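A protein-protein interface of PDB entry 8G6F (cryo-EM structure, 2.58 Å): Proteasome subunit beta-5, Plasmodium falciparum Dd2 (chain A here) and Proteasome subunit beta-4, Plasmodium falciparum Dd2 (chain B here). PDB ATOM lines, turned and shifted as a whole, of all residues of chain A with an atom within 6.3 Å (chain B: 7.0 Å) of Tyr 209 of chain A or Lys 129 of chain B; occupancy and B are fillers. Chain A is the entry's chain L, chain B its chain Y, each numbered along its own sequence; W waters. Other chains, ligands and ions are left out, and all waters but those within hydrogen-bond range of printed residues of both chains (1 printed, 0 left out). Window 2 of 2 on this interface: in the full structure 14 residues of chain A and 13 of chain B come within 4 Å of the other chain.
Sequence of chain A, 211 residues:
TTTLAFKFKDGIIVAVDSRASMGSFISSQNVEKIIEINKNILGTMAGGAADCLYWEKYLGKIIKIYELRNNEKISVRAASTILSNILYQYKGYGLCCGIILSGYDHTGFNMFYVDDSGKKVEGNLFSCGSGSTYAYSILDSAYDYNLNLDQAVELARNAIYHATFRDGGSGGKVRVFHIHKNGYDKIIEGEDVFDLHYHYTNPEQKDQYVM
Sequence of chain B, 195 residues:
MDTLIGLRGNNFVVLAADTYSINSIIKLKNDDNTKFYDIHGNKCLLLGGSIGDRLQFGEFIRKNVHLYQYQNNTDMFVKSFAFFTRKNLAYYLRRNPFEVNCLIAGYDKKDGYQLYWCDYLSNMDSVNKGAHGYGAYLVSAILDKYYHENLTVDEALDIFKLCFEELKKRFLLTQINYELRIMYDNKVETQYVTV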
ATOM      1  N   PHE A 165     -14.276   5.879 -30.754  1.00  0.00           N
ATOM      2  CA  PHE A 165     -14.206   7.037 -29.872  1.00  0.00           C
ATOM      3  C   PHE A 165     -12.828   7.682 -29.907  1.00  0.00           C
ATOM      4  O   PHE A 165     -12.717   8.912 -29.919  1.00  0.00           O
ATOM      5  CB  PHE A 165     -14.565   6.627 -28.448  1.00  0.00           C
ATOM      6  CG  PHE A 165     -14.647   7.777 -27.491  1.00  0.00           C
ATOM      7  CD1 PHE A 165     -15.564   8.792 -27.684  1.00  0.00           C
ATOM      8  CD2 PHE A 165     -13.808   7.845 -26.396  1.00  0.00           C
ATOM      9  CE1 PHE A 165     -15.640   9.847 -26.809  1.00  0.00           C
ATOM     10  CE2 PHE A 165     -13.884   8.899 -25.520  1.00  0.00           C
ATOM     11  CZ  PHE A 165     -14.800   9.902 -25.727  1.00  0.00           C
ATOM     12  N   ARG A 166     -11.768   6.880 -29.917  1.00  0.00           N
ATOM     13  CA  ARG A 166     -10.423   7.441 -29.854  1.00  0.00           C
ATOM     14  C   ARG A 166      -9.835   7.778 -31.217  1.00  0.00           C
ATOM     15  O   ARG A 166      -8.933   8.618 -31.291  1.00  0.00           O
ATOM     16  CB  ARG A 166      -9.480   6.476 -29.136  1.00  0.00           C
ATOM     17  CG  ARG A 166      -9.489   6.624 -27.633  1.00  0.00           C
ATOM     18  CD  ARG A 166      -8.548   7.714 -27.174  1.00  0.00           C
ATOM     19  NE  ARG A 166      -8.628   7.918 -25.734  1.00  0.00           N
ATOM     20  CZ  ARG A 166      -7.981   8.865 -25.071  1.00  0.00           C
ATOM     21  NH1 ARG A 166      -7.187   9.721 -25.689  1.00  0.00           N
ATOM     22  NH2 ARG A 166      -8.130   8.952 -23.754  1.00  0.00           N
ATOM     23  N   HIS A 197     -22.028   5.554 -27.289  1.00  0.00           N
ATOM     24  CA  HIS A 197     -21.318   6.488 -26.420  1.00  0.00           C
ATOM     25  C   HIS A 197     -22.149   6.835 -25.191  1.00  0.00           C
ATOM     26  O   HIS A 197     -21.644   6.834 -24.064  1.00  0.00           O
ATOM     27  CB  HIS A 197     -20.944   7.763 -27.170  1.00  0.00           C
ATOM     28  CG  HIS A 197     -20.406   8.835 -26.275  1.00  0.00           C
ATOM     29  ND1 HIS A 197     -19.087   8.886 -25.885  1.00  0.00           N
ATOM     30  CD2 HIS A 197     -21.016   9.879 -25.667  1.00  0.00           C
ATOM     31  CE1 HIS A 197     -18.903   9.921 -25.087  1.00  0.00           C
ATOM     32  NE2 HIS A 197     -20.059  10.540 -24.939  1.00  0.00           N
ATOM     33  N   THR A 201     -20.259   5.528 -21.873  1.00  0.00           N
ATOM     34  CA  THR A 201     -19.413   6.535 -21.247  1.00  0.00           C
ATOM     35  C   THR A 201     -20.192   7.666 -20.591  1.00  0.00           C
ATOM     36  O   THR A 201     -19.787   8.147 -19.530  1.00  0.00           O
ATOM     37  CB  THR A 201     -18.456   7.117 -22.288  1.00  0.00           C
ATOM     38  OG1 THR A 201     -17.682   6.062 -22.868  1.00  0.00           O
ATOM     39  CG2 THR A 201     -17.531   8.115 -21.659  1.00  0.00           C
ATOM     40  N   ASN A 202     -21.300   8.104 -21.184  1.00  0.00           N
ATOM     41  CA  ASN A 202     -22.084   9.225 -20.665  1.00  0.00           C
ATOM     42  C   ASN A 202     -23.550   8.825 -20.557  1.00  0.00           C
ATOM     43  O   ASN A 202     -24.419   9.404 -21.213  1.00  0.00           O
ATOM     44  CB  ASN A 202     -21.914  10.454 -21.556  1.00  0.00           C
ATOM     45  CG  ASN A 202     -22.164  11.756 -20.817  1.00  0.00           C
ATOM     46  OD1 ASN A 202     -22.370  11.767 -19.608  1.00  0.00           O
ATOM     47  ND2 ASN A 202     -22.146  12.862 -21.547  1.00  0.00           N
ATOM     48  N   ASP A 207     -24.048  16.421 -18.764  1.00  0.00           N
ATOM     49  CA  ASP A 207     -22.958  17.343 -19.046  1.00  0.00           C
ATOM     50  C   ASP A 207     -22.098  16.738 -20.144  1.00  0.00           C
ATOM     51  O   ASP A 207     -22.234  15.565 -20.493  1.00  0.00           O
ATOM     52  CB  ASP A 207     -22.127  17.634 -17.794  1.00  0.00           C
ATOM     53  CG  ASP A 207     -21.703  19.090 -17.701  1.00  0.00           C
ATOM     54  OD1 ASP A 207     -21.451  19.710 -18.757  1.00  0.00           O
ATOM     55  OD2 ASP A 207     -21.622  19.616 -16.572  1.00  0.00           O
ATOM     56  N   GLN A 208     -21.215  17.563 -20.694  1.00  0.00           N
ATOM     57  CA  GLN A 208     -20.276  17.088 -21.698  1.00  0.00           C
ATOM     58  C   GLN A 208     -19.240  16.185 -21.043  1.00  0.00           C
ATOM     59  O   GLN A 208     -18.618  16.560 -20.046  1.00  0.00           O
ATOM     60  CB  GLN A 208     -19.609  18.279 -22.386  1.00  0.00           C
ATOM     61  CG  GLN A 208     -18.350  17.963 -23.182  1.00  0.00           C
ATOM     62  CD  GLN A 208     -18.639  17.245 -24.477  1.00  0.00           C
ATOM     63  OE1 GLN A 208     -19.790  16.991 -24.816  1.00  0.00           O
ATOM     64  NE2 GLN A 208     -17.590  16.915 -25.213  1.00  0.00           N
ATOM     65  N   TYR A 209     -19.055  14.994 -21.602  1.00  0.00           N
ATOM     66  CA  TYR A 209     -18.081  14.062 -21.058  1.00  0.00           C
ATOM     67  C   TYR A 209     -16.670  14.600 -21.246  1.00  0.00           C
ATOM     68  O   TYR A 209     -16.328  15.135 -22.302  1.00  0.00           O
ATOM     69  CB  TYR A 209     -18.214  12.700 -21.732  1.00  0.00           C
ATOM     70  CG  TYR A 209     -17.122  11.735 -21.352  1.00  0.00           C
ATOM     71  CD1 TYR A 209     -17.112  11.122 -20.110  1.00  0.00           C
ATOM     72  CD2 TYR A 209     -16.093  11.444 -22.233  1.00  0.00           C
ATOM     73  CE1 TYR A 209     -16.113  10.245 -19.762  1.00  0.00           C
ATOM     74  CE2 TYR A 209     -15.092  10.570 -21.893  1.00  0.00           C
ATOM     75  CZ  TYR A 209     -15.105   9.972 -20.657  1.00  0.00           C
ATOM     76  OH  TYR A 209     -14.103   9.096 -20.317  1.00  0.00           O
ATOM     77  N   VAL A 210     -15.843  14.445 -20.216  1.00  0.00           N
ATOM     78  CA  VAL A 210     -14.480  14.960 -20.211  1.00  0.00           C
ATOM     79  C   VAL A 210     -13.535  13.778 -20.371  1.00  0.00           C
ATOM     80  O   VAL A 210     -13.433  12.926 -19.481  1.00  0.00           O
ATOM     81  CB  VAL A 210     -14.174  15.746 -18.930  1.00  0.00           C
ATOM     82  CG1 VAL A 210     -12.698  16.079 -18.851  1.00  0.00           C
ATOM     83  CG2 VAL A 210     -15.006  17.008 -18.876  1.00  0.00           C
ATOM     84  N   MET A 211     -12.838  13.729 -21.498  1.00  0.00           N
ATOM     85  CA  MET A 211     -11.806  12.730 -21.726  1.00  0.00           C
ATOM     86  C   MET A 211     -10.477  13.261 -21.184  1.00  0.00           C
ATOM     87  O   MET A 211      -9.840  12.638 -20.336  1.00  0.00           O
ATOM     88  CB  MET A 211     -11.699  12.400 -23.218  1.00  0.00           C
ATOM     89  CG  MET A 211     -10.453  11.629 -23.632  1.00  0.00           C
ATOM     90  SD  MET A 211     -10.068  11.799 -25.380  1.00  0.00           S
ATOM     91  CE  MET A 211     -11.486  11.021 -26.129  1.00  0.00           C
ATOM     92  N   ILE B   5       1.933   7.724 -18.783  1.00  0.00           N
ATOM     93  CA  ILE B   5       0.513   7.532 -18.526  1.00  0.00           C
ATOM     94  C   ILE B   5       0.125   8.379 -17.325  1.00  0.00           C
ATOM     95  O   ILE B   5       0.888   8.489 -16.362  1.00  0.00           O
ATOM     96  CB  ILE B   5       0.166   6.049 -18.281  1.00  0.00           C
ATOM     97  CG1 ILE B   5       0.921   5.148 -19.257  1.00  0.00           C
ATOM     98  CG2 ILE B   5      -1.318   5.828 -18.426  1.00  0.00           C
ATOM     99  CD1 ILE B   5       0.662   3.680 -19.059  1.00  0.00           C
ATOM    100  N   GLY B   6      -1.052   8.988 -17.385  1.00  0.00           N
ATOM    101  CA  GLY B   6      -1.523   9.814 -16.295  1.00  0.00           C
ATOM    102  C   GLY B   6      -3.006   9.644 -16.068  1.00  0.00           C
ATOM    103  O   GLY B   6      -3.779   9.608 -17.025  1.00  0.00           O
ATOM    104  N   LEU B   7      -3.410   9.540 -14.806  1.00  0.00           N
ATOM    105  CA  LEU B   7      -4.801   9.329 -14.438  1.00  0.00           C
ATOM    106  C   LEU B   7      -5.161  10.263 -13.299  1.00  0.00           C
ATOM    107  O   LEU B   7      -4.457  10.312 -12.288  1.00  0.00           O
ATOM    108  CB  LEU B   7      -5.045   7.879 -14.016  1.00  0.00           C
ATOM    109  CG  LEU B   7      -6.501   7.428 -14.030  1.00  0.00           C
ATOM    110  CD1 LEU B   7      -6.945   7.154 -15.447  1.00  0.00           C
ATOM    111  CD2 LEU B   7      -6.677   6.209 -13.164  1.00  0.00           C
ATOM    112  N   ARG B   8      -6.260  10.992 -13.456  1.00  0.00           N
ATOM    113  CA  ARG B   8      -6.717  11.950 -12.464  1.00  0.00           C
ATOM    114  C   ARG B   8      -8.071  11.517 -11.932  1.00  0.00           C
ATOM    115  O   ARG B   8      -9.006  11.293 -12.707  1.00  0.00           O
ATOM    116  CB  ARG B   8      -6.811  13.354 -13.056  1.00  0.00           C
ATOM    117  CG  ARG B   8      -6.991  14.448 -12.028  1.00  0.00           C
ATOM    118  CD  ARG B   8      -7.885  15.544 -12.554  1.00  0.00           C
ATOM    119  NE  ARG B   8      -9.267  15.106 -12.676  1.00  0.00           N
ATOM    120  CZ  ARG B   8     -10.185  15.227 -11.728  1.00  0.00           C
ATOM    121  NH1 ARG B   8      -9.911  15.788 -10.563  1.00  0.00           N
ATOM    122  NH2 ARG B   8     -11.411  14.765 -11.952  1.00  0.00           N
ATOM    123  N   LEU B 103       3.504  15.480 -18.948  1.00  0.00           N
ATOM    124  CA  LEU B 103       2.329  15.262 -18.118  1.00  0.00           C
ATOM    125  C   LEU B 103       2.560  16.017 -16.821  1.00  0.00           C
ATOM    126  O   LEU B 103       3.488  15.701 -16.074  1.00  0.00           O
ATOM    127  CB  LEU B 103       2.093  13.774 -17.852  1.00  0.00           C
ATOM    128  CG  LEU B 103       1.551  12.940 -19.012  1.00  0.00           C
ATOM    129  CD1 LEU B 103       1.609  11.478 -18.663  1.00  0.00           C
ATOM    130  CD2 LEU B 103       0.137  13.334 -19.369  1.00  0.00           C
ATOM    131  N   LEU B 115      -4.397  17.282 -13.617  1.00  0.00           N
ATOM    132  CA  LEU B 115      -3.527  16.631 -14.584  1.00  0.00           C
ATOM    133  C   LEU B 115      -3.642  17.364 -15.911  1.00  0.00           C
ATOM    134  O   LEU B 115      -4.750  17.617 -16.387  1.00  0.00           O
ATOM    135  CB  LEU B 115      -3.907  15.156 -14.758  1.00  0.00           C
ATOM    136  CG  LEU B 115      -3.188  14.371 -15.853  1.00  0.00           C
ATOM    137  CD1 LEU B 115      -1.750  14.091 -15.463  1.00  0.00           C
ATOM    138  CD2 LEU B 115      -3.929  13.087 -16.134  1.00  0.00           C
ATOM    139  N   TRP B 117      -2.050  17.542 -19.996  1.00  0.00           N
ATOM    140  CA  TRP B 117      -1.403  16.827 -21.086  1.00  0.00           C
ATOM    141  C   TRP B 117      -0.813  17.858 -22.037  1.00  0.00           C
ATOM    142  O   TRP B 117      -1.516  18.780 -22.452  1.00  0.00           O
ATOM    143  CB  TRP B 117      -2.431  15.941 -21.796  1.00  0.00           C
ATOM    144  CG  TRP B 117      -1.947  15.132 -22.961  1.00  0.00           C
ATOM    145  CD1 TRP B 117      -1.621  13.813 -22.955  1.00  0.00           C
ATOM    146  CD2 TRP B 117      -1.779  15.579 -24.310  1.00  0.00           C
ATOM    147  NE1 TRP B 117      -1.248  13.412 -24.208  1.00  0.00           N
ATOM    148  CE2 TRP B 117      -1.334  14.479 -25.059  1.00  0.00           C
ATOM    149  CE3 TRP B 117      -1.950  16.806 -24.953  1.00  0.00           C
ATOM    150  CZ2 TRP B 117      -1.056  14.567 -26.416  1.00  0.00           C
ATOM    151  CZ3 TRP B 117      -1.673  16.890 -26.295  1.00  0.00           C
ATOM    152  CH2 TRP B 117      -1.237  15.777 -27.016  1.00  0.00           C
ATOM    153  N   SER B 126      -6.130  20.371 -19.846  1.00  0.00           N
ATOM    154  CA  SER B 126      -6.361  19.583 -18.647  1.00  0.00           C
ATOM    155  C   SER B 126      -7.251  18.395 -18.974  1.00  0.00           C
ATOM    156  O   SER B 126      -8.261  18.528 -19.666  1.00  0.00           O
ATOM    157  CB  SER B 126      -7.003  20.437 -17.557  1.00  0.00           C
ATOM    158  OG  SER B 126      -8.354  20.714 -17.854  1.00  0.00           O
ATOM    159  N   VAL B 127      -6.866  17.224 -18.471  1.00  0.00           N
ATOM    160  CA  VAL B 127      -7.529  15.973 -18.806  1.00  0.00           C
ATOM    161  C   VAL B 127      -7.716  15.150 -17.542  1.00  0.00           C
ATOM    162  O   VAL B 127      -7.093  15.400 -16.510  1.00  0.00           O
ATOM    163  CB  VAL B 127      -6.734  15.169 -19.854  1.00  0.00           C
ATOM    164  CG1 VAL B 127      -6.808  15.854 -21.201  1.00  0.00           C
ATOM    165  CG2 VAL B 127      -5.291  15.000 -19.417  1.00  0.00           C
ATOM    166  N   ASN B 128      -8.610  14.169 -17.632  1.00  0.00           N
ATOM    167  CA  ASN B 128      -8.762  13.170 -16.585  1.00  0.00           C
ATOM    168  C   ASN B 128      -7.847  11.975 -16.788  1.00  0.00           C
ATOM    169  O   ASN B 128      -7.517  11.289 -15.818  1.00  0.00           O
ATOM    170  CB  ASN B 128     -10.210  12.679 -16.519  1.00  0.00           C
ATOM    171  CG  ASN B 128     -11.133  13.683 -15.879  1.00  0.00           C
ATOM    172  OD1 ASN B 128     -10.768  14.350 -14.916  1.00  0.00           O
ATOM    173  ND2 ASN B 128     -12.339  13.802 -16.413  1.00  0.00           N
ATOM    174  N   LYS B 129      -7.442  11.710 -18.023  1.00  0.00           N
ATOM    175  CA  LYS B 129      -6.510  10.637 -18.314  1.00  0.00           C
ATOM    176  C   LYS B 129      -5.787  10.974 -19.604  1.00  0.00           C
ATOM    177  O   LYS B 129      -6.388  11.511 -20.536  1.00  0.00           O
ATOM    178  CB  LYS B 129      -7.227   9.289 -18.425  1.00  0.00           C
ATOM    179  CG  LYS B 129      -8.141   9.165 -19.616  1.00  0.00           C
ATOM    180  CD  LYS B 129      -9.258   8.186 -19.345  1.00  0.00           C
ATOM    181  CE  LYS B 129     -10.464   8.868 -18.750  1.00  0.00           C
ATOM    182  NZ  LYS B 129     -11.216   9.638 -19.765  1.00  0.00           N
ATOM    183  N   GLY B 130      -4.495  10.664 -19.649  1.00  0.00           N
ATOM    184  CA  GLY B 130      -3.684  10.984 -20.806  1.00  0.00           C
ATOM    185  C   GLY B 130      -2.519  10.031 -20.942  1.00  0.00           C
ATOM    186  O   GLY B 130      -2.175   9.298 -20.017  1.00  0.00           O
ATOM    187  N   ALA B 131      -1.908  10.051 -22.121  1.00  0.00           N
ATOM    188  CA  ALA B 131      -0.768   9.192 -22.386  1.00  0.00           C
ATOM    189  C   ALA B 131       0.100   9.805 -23.472  1.00  0.00           C
ATOM    190  O   ALA B 131      -0.370  10.581 -24.306  1.00  0.00           O
ATOM    191  CB  ALA B 131      -1.213   7.787 -22.798  1.00  0.00           C
ATOM    192  N   SER B 140      -4.598   4.055 -24.130  1.00  0.00           N
ATOM    193  CA  SER B 140      -5.625   5.087 -24.045  1.00  0.00           C
ATOM    194  C   SER B 140      -7.017   4.487 -23.938  1.00  0.00           C
ATOM    195  O   SER B 140      -7.845   4.959 -23.153  1.00  0.00           O
ATOM    196  CB  SER B 140      -5.534   6.002 -25.262  1.00  0.00           C
ATOM    197  OG  SER B 140      -4.356   6.779 -25.220  1.00  0.00           O
ATOM    198  N   ILE B 142      -7.822   1.473 -22.809  1.00  0.00           N
ATOM    199  CA  ILE B 142      -7.973   0.838 -21.501  1.00  0.00           C
ATOM    200  C   ILE B 142      -8.338   1.884 -20.459  1.00  0.00           C
ATOM    201  O   ILE B 142      -9.241   1.684 -19.634  1.00  0.00           O
ATOM    202  CB  ILE B 142      -6.685   0.090 -21.111  1.00  0.00           C
ATOM    203  CG1 ILE B 142      -6.401  -1.045 -22.088  1.00  0.00           C
ATOM    204  CG2 ILE B 142      -6.791  -0.458 -19.692  1.00  0.00           C
ATOM    205  CD1 ILE B 142      -4.990  -1.559 -22.015  1.00  0.00           C
ATOM    206  N   LEU B 143      -7.634   3.017 -20.479  1.00  0.00           N
ATOM    207  CA  LEU B 143      -7.962   4.103 -19.562  1.00  0.00           C
ATOM    208  C   LEU B 143      -9.402   4.556 -19.751  1.00  0.00           C
ATOM    209  O   LEU B 143     -10.159   4.678 -18.783  1.00  0.00           O
ATOM    210  CB  LEU B 143      -7.003   5.272 -19.777  1.00  0.00           C
ATOM    211  CG  LEU B 143      -5.544   5.038 -19.395  1.00  0.00           C
ATOM    212  CD1 LEU B 143      -4.712   6.250 -19.741  1.00  0.00           C
ATOM    213  CD2 LEU B 143      -5.429   4.711 -17.926  1.00  0.00           C
ATOM    214  N   ASP B 144      -9.801   4.794 -21.002  1.00  0.00           N
ATOM    215  CA  ASP B 144     -11.168   5.212 -21.290  1.00  0.00           C
ATOM    216  C   ASP B 144     -12.176   4.223 -20.725  1.00  0.00           C
ATOM    217  O   ASP B 144     -13.143   4.610 -20.061  1.00  0.00           O
ATOM    218  CB  ASP B 144     -11.366   5.348 -22.799  1.00  0.00           C
ATOM    219  CG  ASP B 144     -10.713   6.584 -23.368  1.00  0.00           C
ATOM    220  OD1 ASP B 144     -10.452   7.534 -22.605  1.00  0.00           O
ATOM    221  OD2 ASP B 144     -10.459   6.605 -24.587  1.00  0.00           O
ATOM    222  N   LYS B 145     -11.964   2.934 -20.985  1.00  0.00           N
ATOM    223  CA  LYS B 145     -12.948   1.926 -20.614  1.00  0.00           C
ATOM    224  C   LYS B 145     -13.074   1.797 -19.105  1.00  0.00           C
ATOM    225  O   LYS B 145     -14.184   1.799 -18.564  1.00  0.00           O
ATOM    226  CB  LYS B 145     -12.574   0.580 -21.226  1.00  0.00           C
ATOM    227  CG  LYS B 145     -13.683  -0.441 -21.161  1.00  0.00           C
ATOM    228  CD  LYS B 145     -13.192  -1.821 -21.510  1.00  0.00           C
ATOM    229  CE  LYS B 145     -14.144  -2.884 -21.008  1.00  0.00           C
ATOM    230  NZ  LYS B 145     -14.218  -4.039 -21.933  1.00  0.00           N
ATOM    231  N   TYR B 147     -11.864   3.737 -16.603  1.00  0.00           N
ATOM    232  CA  TYR B 147     -11.964   4.929 -15.779  1.00  0.00           C
ATOM    233  C   TYR B 147     -13.418   5.228 -15.452  1.00  0.00           C
ATOM    234  O   TYR B 147     -14.305   5.077 -16.294  1.00  0.00           O
ATOM    235  CB  TYR B 147     -11.340   6.122 -16.497  1.00  0.00           C
ATOM    236  CG  TYR B 147     -11.401   7.418 -15.725  1.00  0.00           C
ATOM    237  CD1 TYR B 147     -12.505   8.249 -15.810  1.00  0.00           C
ATOM    238  CD2 TYR B 147     -10.345   7.821 -14.926  1.00  0.00           C
ATOM    239  CE1 TYR B 147     -12.559   9.430 -15.114  1.00  0.00           C
ATOM    240  CE2 TYR B 147     -10.392   9.003 -14.229  1.00  0.00           C
ATOM    241  CZ  TYR B 147     -11.499   9.802 -14.328  1.00  0.00           C
ATOM    242  OH  TYR B 147     -11.547  10.981 -13.629  1.00  0.00           O
ATOM    243  N   HIS B 148     -13.655   5.651 -14.215  1.00  0.00           N
ATOM    244  CA  HIS B 148     -14.947   6.190 -13.826  1.00  0.00           C
ATOM    245  C   HIS B 148     -14.722   7.192 -12.707  1.00  0.00           C
ATOM    246  O   HIS B 148     -13.672   7.202 -12.062  1.00  0.00           O
ATOM    247  CB  HIS B 148     -15.924   5.090 -13.395  1.00  0.00           C
ATOM    248  CG  HIS B 148     -15.528   4.379 -12.139  1.00  0.00           C
ATOM    249  ND1 HIS B 148     -15.816   4.869 -10.884  1.00  0.00           N
ATOM    250  CD2 HIS B 148     -14.880   3.206 -11.945  1.00  0.00           C
ATOM    251  CE1 HIS B 148     -15.355   4.032  -9.972  1.00  0.00           C
ATOM    252  NE2 HIS B 148     -14.783   3.015 -10.589  1.00  0.00           N
ATOM    253  N   GLU B 149     -15.709   8.056 -12.505  1.00  0.00           N
ATOM    254  CA  GLU B 149     -15.652   8.988 -11.391  1.00  0.00           C
ATOM    255  C   GLU B 149     -15.859   8.243 -10.080  1.00  0.00           C
ATOM    256  O   GLU B 149     -16.558   7.228 -10.019  1.00  0.00           O
ATOM    257  CB  GLU B 149     -16.709  10.081 -11.549  1.00  0.00           C
ATOM    258  CG  GLU B 149     -16.417  11.099 -12.644  1.00  0.00           C
ATOM    259  CD  GLU B 149     -15.040  11.717 -12.526  1.00  0.00           C
ATOM    260  OE1 GLU B 149     -14.486  11.729 -11.409  1.00  0.00           O
ATOM    261  OE2 GLU B 149     -14.514  12.199 -13.550  1.00  0.00           O
HETATM  262  O   HOH W   1     -14.676  11.487 -16.968  1.00  0.00           O
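Water W1 lies within hydrogen-bond range of O of Val 210 of chain A (3.2 Å), ND2 of Asn 128 of chain B (3.3 Å) and OE2 of Glu 149 of chain B (3.5 Å).
Tyr 209 of chain A touches one residue of chain B.
Lys 129 of chain B touches just these residues of chain A: Tyr 209 (3.0 Å), Val 210 (3.98 Å) and Met 211 (3.3 Å).
Of the printed residues of chain B, Val 210 of chain A touches Asn 128 and Lys 129.
Of the printed residues of chain A, Ser 140 of chain B touches Arg 166 (3.7 Å).
Leu 103 of chain B touches none of the printed residues of chain A.
The nearest residue of chain B that does not touch Tyr 209 of chain A is Asp 144 of chain B (4.6 Å).
The nearest residue of chain A that does not touch Lys 129 of chain B is Arg 166 of chain A (4.1 Å).
Among the printed residues, pairs that only touch across the chains: Arg 166 of chain A with Ser 140 of chain B and Val 210 of chain A with Lys 129 of chain B.
Of the 10 printed residues of chain A, 4 touch a printed residue of chain B.
Printed residues of chain A that touch a printed residue of chain B: Arg 166, Tyr 209, Val 210 and Met 211.
Hydrophobic or aromatic side chains of chain A within 4 Å of the printed part of chain B: Tyr 209 and Val 210.
Printed residues of chain B that touch a printed residue of chain A: Asn 128, Lys 129, Ser 140 and Asp 144.
Along chain B the printed residues that touch a printed residue of chain A span positions 128 to 144.
Among the printed residues, 7 pairs touch across the chains.
The side-chain carboxylate (OD2) of Asp 144 of chain B is in salt-bridge range of the guanidinium group (NE) of Arg 166 of chain A, 2.5 Å away.
The side-chain amino group of Lys 129 of chain B is in hydrogen-bond range of the side-chain hydroxyl of Tyr 209 of chain A (3.0 Å).
The side-chain amino group (NZ) of Lys 129 of chain B lies within hydrogen-bond range of the backbone carbonyl oxygen (O) of Met 211 of chain A (3.3 Å).
ND2 of Asn 128 of chain B lies close to O of Val 210 of chain A, at 3.4 Å.
N of Asn 128 of chain B sits at hydrogen-bond distance from O of Met 211 of chain A, 3.3 Å away.
The backbone NH of Arg 8 of chain B sits at hydrogen-bond distance from the backbone carbonyl oxygen of Asn 128 of chain B, 2.7 Å away.
NZ of Lys 129 of chain B is in salt-bridge range of OD1 of Asp 144 of chain B, at 3.6 Å.
The guanidinium group (NH1) of Arg 166 of chain A is in hydrogen-bond range of the side-chain sulfur (SD) of Met 211 of chain A (3.6 Å).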
